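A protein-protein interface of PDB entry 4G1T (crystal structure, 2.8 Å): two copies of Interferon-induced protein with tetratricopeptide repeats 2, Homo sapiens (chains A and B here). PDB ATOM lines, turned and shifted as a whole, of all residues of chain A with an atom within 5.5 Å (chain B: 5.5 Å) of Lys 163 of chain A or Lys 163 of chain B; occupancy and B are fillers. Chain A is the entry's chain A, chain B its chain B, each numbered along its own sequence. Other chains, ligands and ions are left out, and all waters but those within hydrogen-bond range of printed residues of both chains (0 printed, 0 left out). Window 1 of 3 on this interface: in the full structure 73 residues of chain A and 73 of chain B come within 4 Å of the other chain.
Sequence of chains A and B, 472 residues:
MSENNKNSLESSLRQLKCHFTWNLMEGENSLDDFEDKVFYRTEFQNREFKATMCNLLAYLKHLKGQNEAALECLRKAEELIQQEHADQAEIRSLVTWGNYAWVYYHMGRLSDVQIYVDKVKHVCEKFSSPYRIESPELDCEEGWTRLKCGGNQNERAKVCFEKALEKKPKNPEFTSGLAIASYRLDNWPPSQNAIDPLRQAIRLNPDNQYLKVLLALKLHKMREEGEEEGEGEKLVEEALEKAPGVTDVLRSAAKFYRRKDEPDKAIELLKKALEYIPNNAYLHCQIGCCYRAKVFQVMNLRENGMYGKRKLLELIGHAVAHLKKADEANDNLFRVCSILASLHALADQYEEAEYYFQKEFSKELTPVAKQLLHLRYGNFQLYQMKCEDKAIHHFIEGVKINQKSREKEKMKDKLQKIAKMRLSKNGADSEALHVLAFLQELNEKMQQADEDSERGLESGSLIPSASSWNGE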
ATOM      1  N   LYS A  17     -13.782   7.923 -16.445  1.00  0.00           N
ATOM      2  CA  LYS A  17     -12.515   7.342 -16.865  1.00  0.00           C
ATOM      3  C   LYS A  17     -12.162   7.819 -18.265  1.00  0.00           C
ATOM      4  O   LYS A  17     -12.796   7.426 -19.245  1.00  0.00           O
ATOM      5  CB  LYS A  17     -12.580   5.799 -16.900  1.00  0.00           C
ATOM      6  CG  LYS A  17     -12.488   5.068 -15.565  1.00  0.00           C
ATOM      7  CD  LYS A  17     -12.451   3.564 -15.811  1.00  0.00           C
ATOM      8  CE  LYS A  17     -12.305   2.758 -14.528  1.00  0.00           C
ATOM      9  NZ  LYS A  17     -11.969   1.333 -14.824  1.00  0.00           N
ATOM     10  N   PRO A 136     -11.691   3.821  -3.311  1.00  0.00           N
ATOM     11  CA  PRO A 136     -10.408   4.045  -2.660  1.00  0.00           C
ATOM     12  C   PRO A 136     -10.232   2.938  -1.618  1.00  0.00           C
ATOM     13  O   PRO A 136      -9.179   2.307  -1.569  1.00  0.00           O
ATOM     14  CB  PRO A 136     -10.610   5.397  -1.974  1.00  0.00           C
ATOM     15  CG  PRO A 136     -12.086   5.452  -1.704  1.00  0.00           C
ATOM     16  CD  PRO A 136     -12.685   4.845  -2.935  1.00  0.00           C
ATOM     17  N   ASP A 139      -9.282  -0.350  -3.164  1.00  0.00           N
ATOM     18  CA  ASP A 139      -7.903  -0.309  -3.610  1.00  0.00           C
ATOM     19  C   ASP A 139      -6.937  -0.360  -2.432  1.00  0.00           C
ATOM     20  O   ASP A 139      -5.825  -0.865  -2.563  1.00  0.00           O
ATOM     21  CB  ASP A 139      -7.659   0.937  -4.463  1.00  0.00           C
ATOM     22  CG  ASP A 139      -8.267   0.819  -5.845  1.00  0.00           C
ATOM     23  OD1 ASP A 139      -9.271   0.083  -6.010  1.00  0.00           O
ATOM     24  OD2 ASP A 139      -7.738   1.465  -6.772  1.00  0.00           O
ATOM     25  N   LYS A 158       1.909  -0.391  -4.540  1.00  0.00           N
ATOM     26  CA  LYS A 158       2.098   1.056  -4.667  1.00  0.00           C
ATOM     27  C   LYS A 158       1.010   1.672  -5.535  1.00  0.00           C
ATOM     28  O   LYS A 158       0.335   2.615  -5.127  1.00  0.00           O
ATOM     29  CB  LYS A 158       3.463   1.382  -5.266  1.00  0.00           C
ATOM     30  CG  LYS A 158       3.864   2.835  -5.110  1.00  0.00           C
ATOM     31  CD  LYS A 158       5.150   3.154  -5.854  1.00  0.00           C
ATOM     32  CE  LYS A 158       4.934   3.055  -7.346  1.00  0.00           C
ATOM     33  NZ  LYS A 158       6.216   3.158  -8.076  1.00  0.00           N
ATOM     34  N   VAL A 159       0.846   1.129  -6.733  1.00  0.00           N
ATOM     35  CA  VAL A 159      -0.247   1.528  -7.605  1.00  0.00           C
ATOM     36  C   VAL A 159      -1.569   1.564  -6.830  1.00  0.00           C
ATOM     37  O   VAL A 159      -2.288   2.559  -6.873  1.00  0.00           O
ATOM     38  CB  VAL A 159      -0.352   0.595  -8.828  1.00  0.00           C
ATOM     39  CG1 VAL A 159      -1.633   0.867  -9.585  1.00  0.00           C
ATOM     40  CG2 VAL A 159       0.880   0.739  -9.727  1.00  0.00           C
ATOM     41  N   CYS A 160      -1.879   0.491  -6.109  1.00  0.00           N
ATOM     42  CA  CYS A 160      -3.089   0.438  -5.298  1.00  0.00           C
ATOM     43  C   CYS A 160      -3.244   1.692  -4.437  1.00  0.00           C
ATOM     44  O   CYS A 160      -4.303   2.308  -4.415  1.00  0.00           O
ATOM     45  CB  CYS A 160      -3.101  -0.799  -4.390  1.00  0.00           C
ATOM     46  SG  CYS A 160      -3.541  -2.372  -5.166  1.00  0.00           S
ATOM     47  N   PHE A 161      -2.187   2.069  -3.725  1.00  0.00           N
ATOM     48  CA  PHE A 161      -2.258   3.225  -2.835  1.00  0.00           C
ATOM     49  C   PHE A 161      -2.284   4.528  -3.640  1.00  0.00           C
ATOM     50  O   PHE A 161      -2.915   5.513  -3.240  1.00  0.00           O
ATOM     51  CB  PHE A 161      -1.119   3.224  -1.799  1.00  0.00           C
ATOM     52  CG  PHE A 161      -1.321   2.241  -0.668  1.00  0.00           C
ATOM     53  CD1 PHE A 161      -2.350   2.411   0.246  1.00  0.00           C
ATOM     54  CD2 PHE A 161      -0.479   1.150  -0.518  1.00  0.00           C
ATOM     55  CE1 PHE A 161      -2.540   1.505   1.287  1.00  0.00           C
ATOM     56  CE2 PHE A 161      -0.665   0.255   0.514  1.00  0.00           C
ATOM     57  CZ  PHE A 161      -1.694   0.430   1.421  1.00  0.00           C
ATOM     58  N   GLU A 162      -1.599   4.526  -4.777  1.00  0.00           N
ATOM     59  CA  GLU A 162      -1.704   5.629  -5.704  1.00  0.00           C
ATOM     60  C   GLU A 162      -3.168   5.824  -6.132  1.00  0.00           C
ATOM     61  O   GLU A 162      -3.730   6.908  -5.955  1.00  0.00           O
ATOM     62  CB  GLU A 162      -0.793   5.403  -6.907  1.00  0.00           C
ATOM     63  CG  GLU A 162       0.669   5.656  -6.610  1.00  0.00           C
ATOM     64  CD  GLU A 162       1.545   5.507  -7.838  1.00  0.00           C
ATOM     65  OE1 GLU A 162       2.748   5.796  -7.737  1.00  0.00           O
ATOM     66  OE2 GLU A 162       1.038   5.109  -8.909  1.00  0.00           O
ATOM     67  N   LYS A 163      -3.789   4.773  -6.665  1.00  0.00           N
ATOM     68  CA  LYS A 163      -5.178   4.857  -7.097  1.00  0.00           C
ATOM     69  C   LYS A 163      -6.115   5.330  -5.993  1.00  0.00           C
ATOM     70  O   LYS A 163      -7.170   5.884  -6.272  1.00  0.00           O
ATOM     71  CB  LYS A 163      -5.680   3.511  -7.619  1.00  0.00           C
ATOM     72  CG  LYS A 163      -5.212   3.150  -9.002  1.00  0.00           C
ATOM     73  CD  LYS A 163      -5.809   1.834  -9.409  1.00  0.00           C
ATOM     74  CE  LYS A 163      -4.960   1.125 -10.475  1.00  0.00           C
ATOM     75  NZ  LYS A 163      -5.270  -0.355 -10.581  1.00  0.00           N
ATOM     76  N   ALA A 164      -5.756   5.087  -4.741  1.00  0.00           N
ATOM     77  CA  ALA A 164      -6.651   5.443  -3.645  1.00  0.00           C
ATOM     78  C   ALA A 164      -6.499   6.905  -3.294  1.00  0.00           C
ATOM     79  O   ALA A 164      -7.389   7.497  -2.685  1.00  0.00           O
ATOM     80  CB  ALA A 164      -6.378   4.586  -2.425  1.00  0.00           C
ATOM     81  N   LEU A 165      -5.357   7.476  -3.672  1.00  0.00           N
ATOM     82  CA  LEU A 165      -5.033   8.858  -3.338  1.00  0.00           C
ATOM     83  C   LEU A 165      -5.457   9.831  -4.440  1.00  0.00           C
ATOM     84  O   LEU A 165      -5.646  11.029  -4.191  1.00  0.00           O
ATOM     85  CB  LEU A 165      -3.548   9.004  -3.000  1.00  0.00           C
ATOM     86  CG  LEU A 165      -3.296   8.819  -1.507  1.00  0.00           C
ATOM     87  CD1 LEU A 165      -1.855   9.152  -1.161  1.00  0.00           C
ATOM     88  CD2 LEU A 165      -4.262   9.671  -0.694  1.00  0.00           C
ATOM     89  N   GLU A 166      -5.606   9.342  -5.665  1.00  0.00           N
ATOM     90  CA  GLU A 166      -6.017  10.247  -6.724  1.00  0.00           C
ATOM     91  C   GLU A 166      -7.404  10.768  -6.371  1.00  0.00           C
ATOM     92  O   GLU A 166      -7.677  11.963  -6.473  1.00  0.00           O
ATOM     93  CB  GLU A 166      -6.047   9.524  -8.071  1.00  0.00           C
ATOM     94  CG  GLU A 166      -4.707   8.945  -8.495  1.00  0.00           C
ATOM     95  CD  GLU A 166      -4.775   8.237  -9.834  1.00  0.00           C
ATOM     96  OE1 GLU A 166      -5.871   8.197 -10.432  1.00  0.00           O
ATOM     97  OE2 GLU A 166      -3.732   7.720 -10.289  1.00  0.00           O
ATOM     98  N   LYS A 167      -8.274   9.854  -5.950  1.00  0.00           N
ATOM     99  CA  LYS A 167      -9.638  10.200  -5.559  1.00  0.00           C
ATOM    100  C   LYS A 167      -9.710  11.042  -4.284  1.00  0.00           C
ATOM    101  O   LYS A 167     -10.477  12.000  -4.202  1.00  0.00           O
ATOM    102  CB  LYS A 167     -10.481   8.932  -5.395  1.00  0.00           C
ATOM    103  CG  LYS A 167     -10.580   8.085  -6.654  1.00  0.00           C
ATOM    104  CD  LYS A 167     -11.425   6.844  -6.419  1.00  0.00           C
ATOM    105  CE  LYS A 167     -11.517   5.992  -7.675  1.00  0.00           C
ATOM    106  NZ  LYS A 167     -12.130   6.739  -8.808  1.00  0.00           N
ATOM    107  N   GLU B 134     -15.829  -0.717 -13.944  1.00  0.00           N
ATOM    108  CA  GLU B 134     -14.617  -1.518 -13.939  1.00  0.00           C
ATOM    109  C   GLU B 134     -14.784  -2.495 -15.066  1.00  0.00           C
ATOM    110  O   GLU B 134     -15.796  -3.147 -15.156  1.00  0.00           O
ATOM    111  CB  GLU B 134     -14.455  -2.251 -12.605  1.00  0.00           C
ATOM    112  CG  GLU B 134     -14.349  -1.311 -11.380  1.00  0.00           C
ATOM    113  CD  GLU B 134     -12.906  -1.080 -10.908  1.00  0.00           C
ATOM    114  OE1 GLU B 134     -11.992  -1.731 -11.464  1.00  0.00           O
ATOM    115  OE2 GLU B 134     -12.686  -0.267  -9.974  1.00  0.00           O
ATOM    116  N   ASP B 139      -9.166  -1.126 -18.973  1.00  0.00           N
ATOM    117  CA  ASP B 139      -7.902  -1.179 -18.272  1.00  0.00           C
ATOM    118  C   ASP B 139      -6.853  -1.295 -19.343  1.00  0.00           C
ATOM    119  O   ASP B 139      -5.760  -0.714 -19.263  1.00  0.00           O
ATOM    120  CB  ASP B 139      -7.870  -2.384 -17.341  1.00  0.00           C
ATOM    121  CG  ASP B 139      -8.562  -2.112 -16.023  1.00  0.00           C
ATOM    122  OD1 ASP B 139      -8.340  -1.018 -15.449  1.00  0.00           O
ATOM    123  OD2 ASP B 139      -9.327  -2.988 -15.564  1.00  0.00           O
ATOM    124  N   ARG B 156       3.018   1.799 -14.206  1.00  0.00           N
ATOM    125  CA  ARG B 156       1.591   2.011 -14.110  1.00  0.00           C
ATOM    126  C   ARG B 156       0.853   1.306 -15.284  1.00  0.00           C
ATOM    127  O   ARG B 156      -0.251   0.780 -15.126  1.00  0.00           O
ATOM    128  CB  ARG B 156       1.351   3.519 -14.083  1.00  0.00           C
ATOM    129  CG  ARG B 156      -0.049   3.939 -13.828  1.00  0.00           C
ATOM    130  CD  ARG B 156      -0.381   3.915 -12.374  1.00  0.00           C
ATOM    131  NE  ARG B 156      -1.830   4.009 -12.190  1.00  0.00           N
ATOM    132  CZ  ARG B 156      -2.448   5.010 -11.568  1.00  0.00           C
ATOM    133  NH1 ARG B 156      -1.747   6.013 -11.045  1.00  0.00           N
ATOM    134  NH2 ARG B 156      -3.769   4.992 -11.452  1.00  0.00           N
ATOM    135  N   LYS B 158       1.946  -1.526 -16.655  1.00  0.00           N
ATOM    136  CA  LYS B 158       1.953  -2.961 -16.388  1.00  0.00           C
ATOM    137  C   LYS B 158       0.722  -3.310 -15.576  1.00  0.00           C
ATOM    138  O   LYS B 158      -0.067  -4.156 -15.984  1.00  0.00           O
ATOM    139  CB  LYS B 158       3.220  -3.453 -15.670  1.00  0.00           C
ATOM    140  CG  LYS B 158       3.421  -4.975 -15.787  1.00  0.00           C
ATOM    141  CD  LYS B 158       4.616  -5.504 -14.985  1.00  0.00           C
ATOM    142  CE  LYS B 158       4.289  -5.608 -13.488  1.00  0.00           C
ATOM    143  NZ  LYS B 158       5.354  -6.262 -12.660  1.00  0.00           N
ATOM    144  N   VAL B 159       0.535  -2.639 -14.449  1.00  0.00           N
ATOM    145  CA  VAL B 159      -0.598  -2.947 -13.602  1.00  0.00           C
ATOM    146  C   VAL B 159      -1.899  -2.958 -14.414  1.00  0.00           C
ATOM    147  O   VAL B 159      -2.787  -3.780 -14.172  1.00  0.00           O
ATOM    148  CB  VAL B 159      -0.715  -1.980 -12.415  1.00  0.00           C
ATOM    149  CG1 VAL B 159      -1.897  -2.349 -11.570  1.00  0.00           C
ATOM    150  CG2 VAL B 159       0.551  -1.987 -11.578  1.00  0.00           C
ATOM    151  N   CYS B 160      -2.016  -2.062 -15.390  1.00  0.00           N
ATOM    152  CA  CYS B 160      -3.258  -1.945 -16.148  1.00  0.00           C
ATOM    153  C   CYS B 160      -3.546  -3.236 -16.879  1.00  0.00           C
ATOM    154  O   CYS B 160      -4.653  -3.744 -16.807  1.00  0.00           O
ATOM    155  CB  CYS B 160      -3.240  -0.746 -17.112  1.00  0.00           C
ATOM    156  SG  CYS B 160      -3.539   0.874 -16.316  1.00  0.00           S
ATOM    157  N   PHE B 161      -2.548  -3.786 -17.562  1.00  0.00           N
ATOM    158  CA  PHE B 161      -2.744  -5.054 -18.270  1.00  0.00           C
ATOM    159  C   PHE B 161      -2.910  -6.230 -17.315  1.00  0.00           C
ATOM    160  O   PHE B 161      -3.687  -7.153 -17.560  1.00  0.00           O
ATOM    161  CB  PHE B 161      -1.597  -5.337 -19.222  1.00  0.00           C
ATOM    162  CG  PHE B 161      -1.482  -4.356 -20.338  1.00  0.00           C
ATOM    163  CD1 PHE B 161      -2.472  -4.255 -21.292  1.00  0.00           C
ATOM    164  CD2 PHE B 161      -0.365  -3.540 -20.449  1.00  0.00           C
ATOM    165  CE1 PHE B 161      -2.361  -3.352 -22.333  1.00  0.00           C
ATOM    166  CE2 PHE B 161      -0.252  -2.645 -21.487  1.00  0.00           C
ATOM    167  CZ  PHE B 161      -1.249  -2.552 -22.433  1.00  0.00           C
ATOM    168  N   GLU B 162      -2.154  -6.204 -16.231  1.00  0.00           N
ATOM    169  CA  GLU B 162      -2.339  -7.189 -15.181  1.00  0.00           C
ATOM    170  C   GLU B 162      -3.797  -7.133 -14.745  1.00  0.00           C
ATOM    171  O   GLU B 162      -4.530  -8.102 -14.924  1.00  0.00           O
ATOM    172  CB  GLU B 162      -1.397  -6.930 -14.011  1.00  0.00           C
ATOM    173  CG  GLU B 162       0.032  -7.308 -14.306  1.00  0.00           C
ATOM    174  CD  GLU B 162       0.959  -7.042 -13.134  1.00  0.00           C
ATOM    175  OE1 GLU B 162       0.533  -6.402 -12.160  1.00  0.00           O
ATOM    176  OE2 GLU B 162       2.121  -7.479 -13.179  1.00  0.00           O
ATOM    177  N   LYS B 163      -4.225  -5.992 -14.213  1.00  0.00           N
ATOM    178  CA  LYS B 163      -5.620  -5.822 -13.815  1.00  0.00           C
ATOM    179  C   LYS B 163      -6.599  -6.351 -14.862  1.00  0.00           C
ATOM    180  O   LYS B 163      -7.658  -6.877 -14.516  1.00  0.00           O
ATOM    181  CB  LYS B 163      -5.930  -4.355 -13.523  1.00  0.00           C
ATOM    182  CG  LYS B 163      -6.328  -4.064 -12.083  1.00  0.00           C
ATOM    183  CD  LYS B 163      -7.024  -2.698 -11.990  1.00  0.00           C
ATOM    184  CE  LYS B 163      -8.446  -2.743 -12.597  1.00  0.00           C
ATOM    185  NZ  LYS B 163      -9.097  -1.407 -12.812  1.00  0.00           N
ATOM    186  N   ALA B 164      -6.251  -6.213 -16.136  1.00  0.00           N
ATOM    187  CA  ALA B 164      -7.123  -6.692 -17.200  1.00  0.00           C
ATOM    188  C   ALA B 164      -7.107  -8.217 -17.273  1.00  0.00           C
ATOM    189  O   ALA B 164      -8.117  -8.827 -17.604  1.00  0.00           O
ATOM    190  CB  ALA B 164      -6.739  -6.086 -18.541  1.00  0.00           C
ATOM    191  N   LEU B 165      -5.963  -8.832 -16.969  1.00  0.00           N
ATOM    192  CA  LEU B 165      -5.843 -10.300 -16.990  1.00  0.00           C
ATOM    193  C   LEU B 165      -6.513 -10.966 -15.784  1.00  0.00           C
ATOM    194  O   LEU B 165      -7.164 -12.004 -15.921  1.00  0.00           O
ATOM    195  CB  LEU B 165      -4.383 -10.730 -17.083  1.00  0.00           C
ATOM    196  CG  LEU B 165      -3.705 -10.452 -18.414  1.00  0.00           C
ATOM    197  CD1 LEU B 165      -2.213 -10.479 -18.213  1.00  0.00           C
ATOM    198  CD2 LEU B 165      -4.142 -11.443 -19.478  1.00  0.00           C
ATOM    199  N   GLU B 166      -6.400 -10.371 -14.605  1.00  0.00           N
ATOM    200  CA  GLU B 166      -7.043 -11.004 -13.469  1.00  0.00           C
ATOM    201  C   GLU B 166      -8.523 -11.071 -13.813  1.00  0.00           C
ATOM    202  O   GLU B 166      -9.166 -12.102 -13.621  1.00  0.00           O
ATOM    203  CB  GLU B 166      -6.827 -10.184 -12.198  1.00  0.00           C
ATOM    204  CG  GLU B 166      -5.366 -10.002 -11.817  1.00  0.00           C
ATOM    205  CD  GLU B 166      -5.192  -9.185 -10.552  1.00  0.00           C
ATOM    206  OE1 GLU B 166      -6.212  -8.760  -9.972  1.00  0.00           O
ATOM    207  OE2 GLU B 166      -4.033  -8.967 -10.139  1.00  0.00           O
ATOM    208  N   LYS B 167      -9.061  -9.971 -14.334  1.00  0.00           N
ATOM    209  CA  LYS B 167     -10.464  -9.932 -14.725  1.00  0.00           C
ATOM    210  C   LYS B 167     -10.734 -10.848 -15.922  1.00  0.00           C
ATOM    211  O   LYS B 167     -11.725 -11.577 -15.952  1.00  0.00           O
ATOM    212  CB  LYS B 167     -10.890  -8.500 -15.052  1.00  0.00           C
ATOM    213  CG  LYS B 167     -10.746  -7.529 -13.891  1.00  0.00           C
ATOM    214  CD  LYS B 167     -11.192  -6.129 -14.283  1.00  0.00           C
ATOM    215  CE  LYS B 167     -11.053  -5.160 -13.121  1.00  0.00           C
ATOM    216  NZ  LYS B 167     -11.488  -3.785 -13.489  1.00  0.00           N
ATOM    217  N   LYS B 168      -9.838 -10.795 -16.906  1.00  0.00           N
ATOM    218  CA  LYS B 168      -9.947 -11.601 -18.123  1.00  0.00           C
ATOM    219  C   LYS B 168      -8.628 -12.270 -18.516  1.00  0.00           C
ATOM    220  O   LYS B 168      -7.972 -11.844 -19.468  1.00  0.00           O
ATOM    221  CB  LYS B 168     -10.467 -10.749 -19.282  1.00  0.00           C
ATOM    222  CG  LYS B 168     -10.682 -11.521 -20.574  1.00  0.00           C
ATOM    223  CD  LYS B 168     -11.244 -10.627 -21.666  1.00  0.00           C
ATOM    224  CE  LYS B 168     -11.436 -11.393 -22.964  1.00  0.00           C
ATOM    225  NZ  LYS B 168     -11.986 -10.528 -24.044  1.00  0.00           N
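The side-chain carboxylate of Glu 166 of chain A is in salt-bridge range of the guanidinium group of Arg 156 of chain B, at 2.7 Å. OE2 of Glu 162 of chain A lies within salt-bridge range of NH1 of Arg 156 of chain B, 3.6 Å away.
The side-chain carboxylate (OE1) of Glu 134 of chain B lies within salt-bridge range of the side-chain amino group (NZ) of Lys 163 of chain B, 3.2 Å away. The side-chain carboxylate (OD1) of Asp 139 of chain B is in salt-bridge range of the side-chain amino group (NZ) of Lys 163 of chain B, at 2.8 Å. O of Arg 156 of chain B is in hydrogen-bond range of SG of Cys 160 of chain B. The side-chain carboxylate of Glu 134 of chain B is in salt-bridge range of the side-chain amino group of Lys 167 of chain B (2.9 Å).
Glu 134 of chain B touches Lys 17 of chain A (CA to NZ, 3.99 Å). CG2 of Val 159 of chain A touches CG2 of Val 159 of chain B, 3.3 Å away. Arg 156 of chain B touches Lys 163 of chain A. CD of Lys 163 of chain B touches NZ of Lys 163 of chain A (3.2 Å).
Of chain B, only Arg 156 (3.4 Å) and Lys 163 (3.2 Å) come within 4 Å of Lys 163 of chain A. Lys 163 of chain B touches just one residue of chain A: Lys 163 (3.2 Å). Of the printed residues of chain A, Glu 134 of chain B touches Lys 17 (3.99 Å). Of the printed residues of chain A, Val 159 of chain B touches Val 159. Of the printed residues of chain A, Arg 156 of chain B touches Glu 162, Lys 163 and Glu 166. Of the printed residues of chain B, Glu 166 of chain A touches Arg 156. The nearest residue of chain B that does not touch Lys 163 of chain A is Val 159 of chain B (4.04 Å). The nearest residue of chain A that does not touch Lys 163 of chain B is Lys 17 of chain A (4.5 Å).
Of the 14 printed residues of chain B, 4 touch a printed residue of chain A. Hydrophobic or aromatic side chains of chain B within 4 Å of the printed part of chain A: Val 159. Hydrophobic or aromatic side chains of chain A that line the printed part of chain B: Val 159.
Val 159 of chain B touches its own counterpart, Val 159 of chain A. Lys 163 of chain B touches its own counterpart, Lys 163 of chain A.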
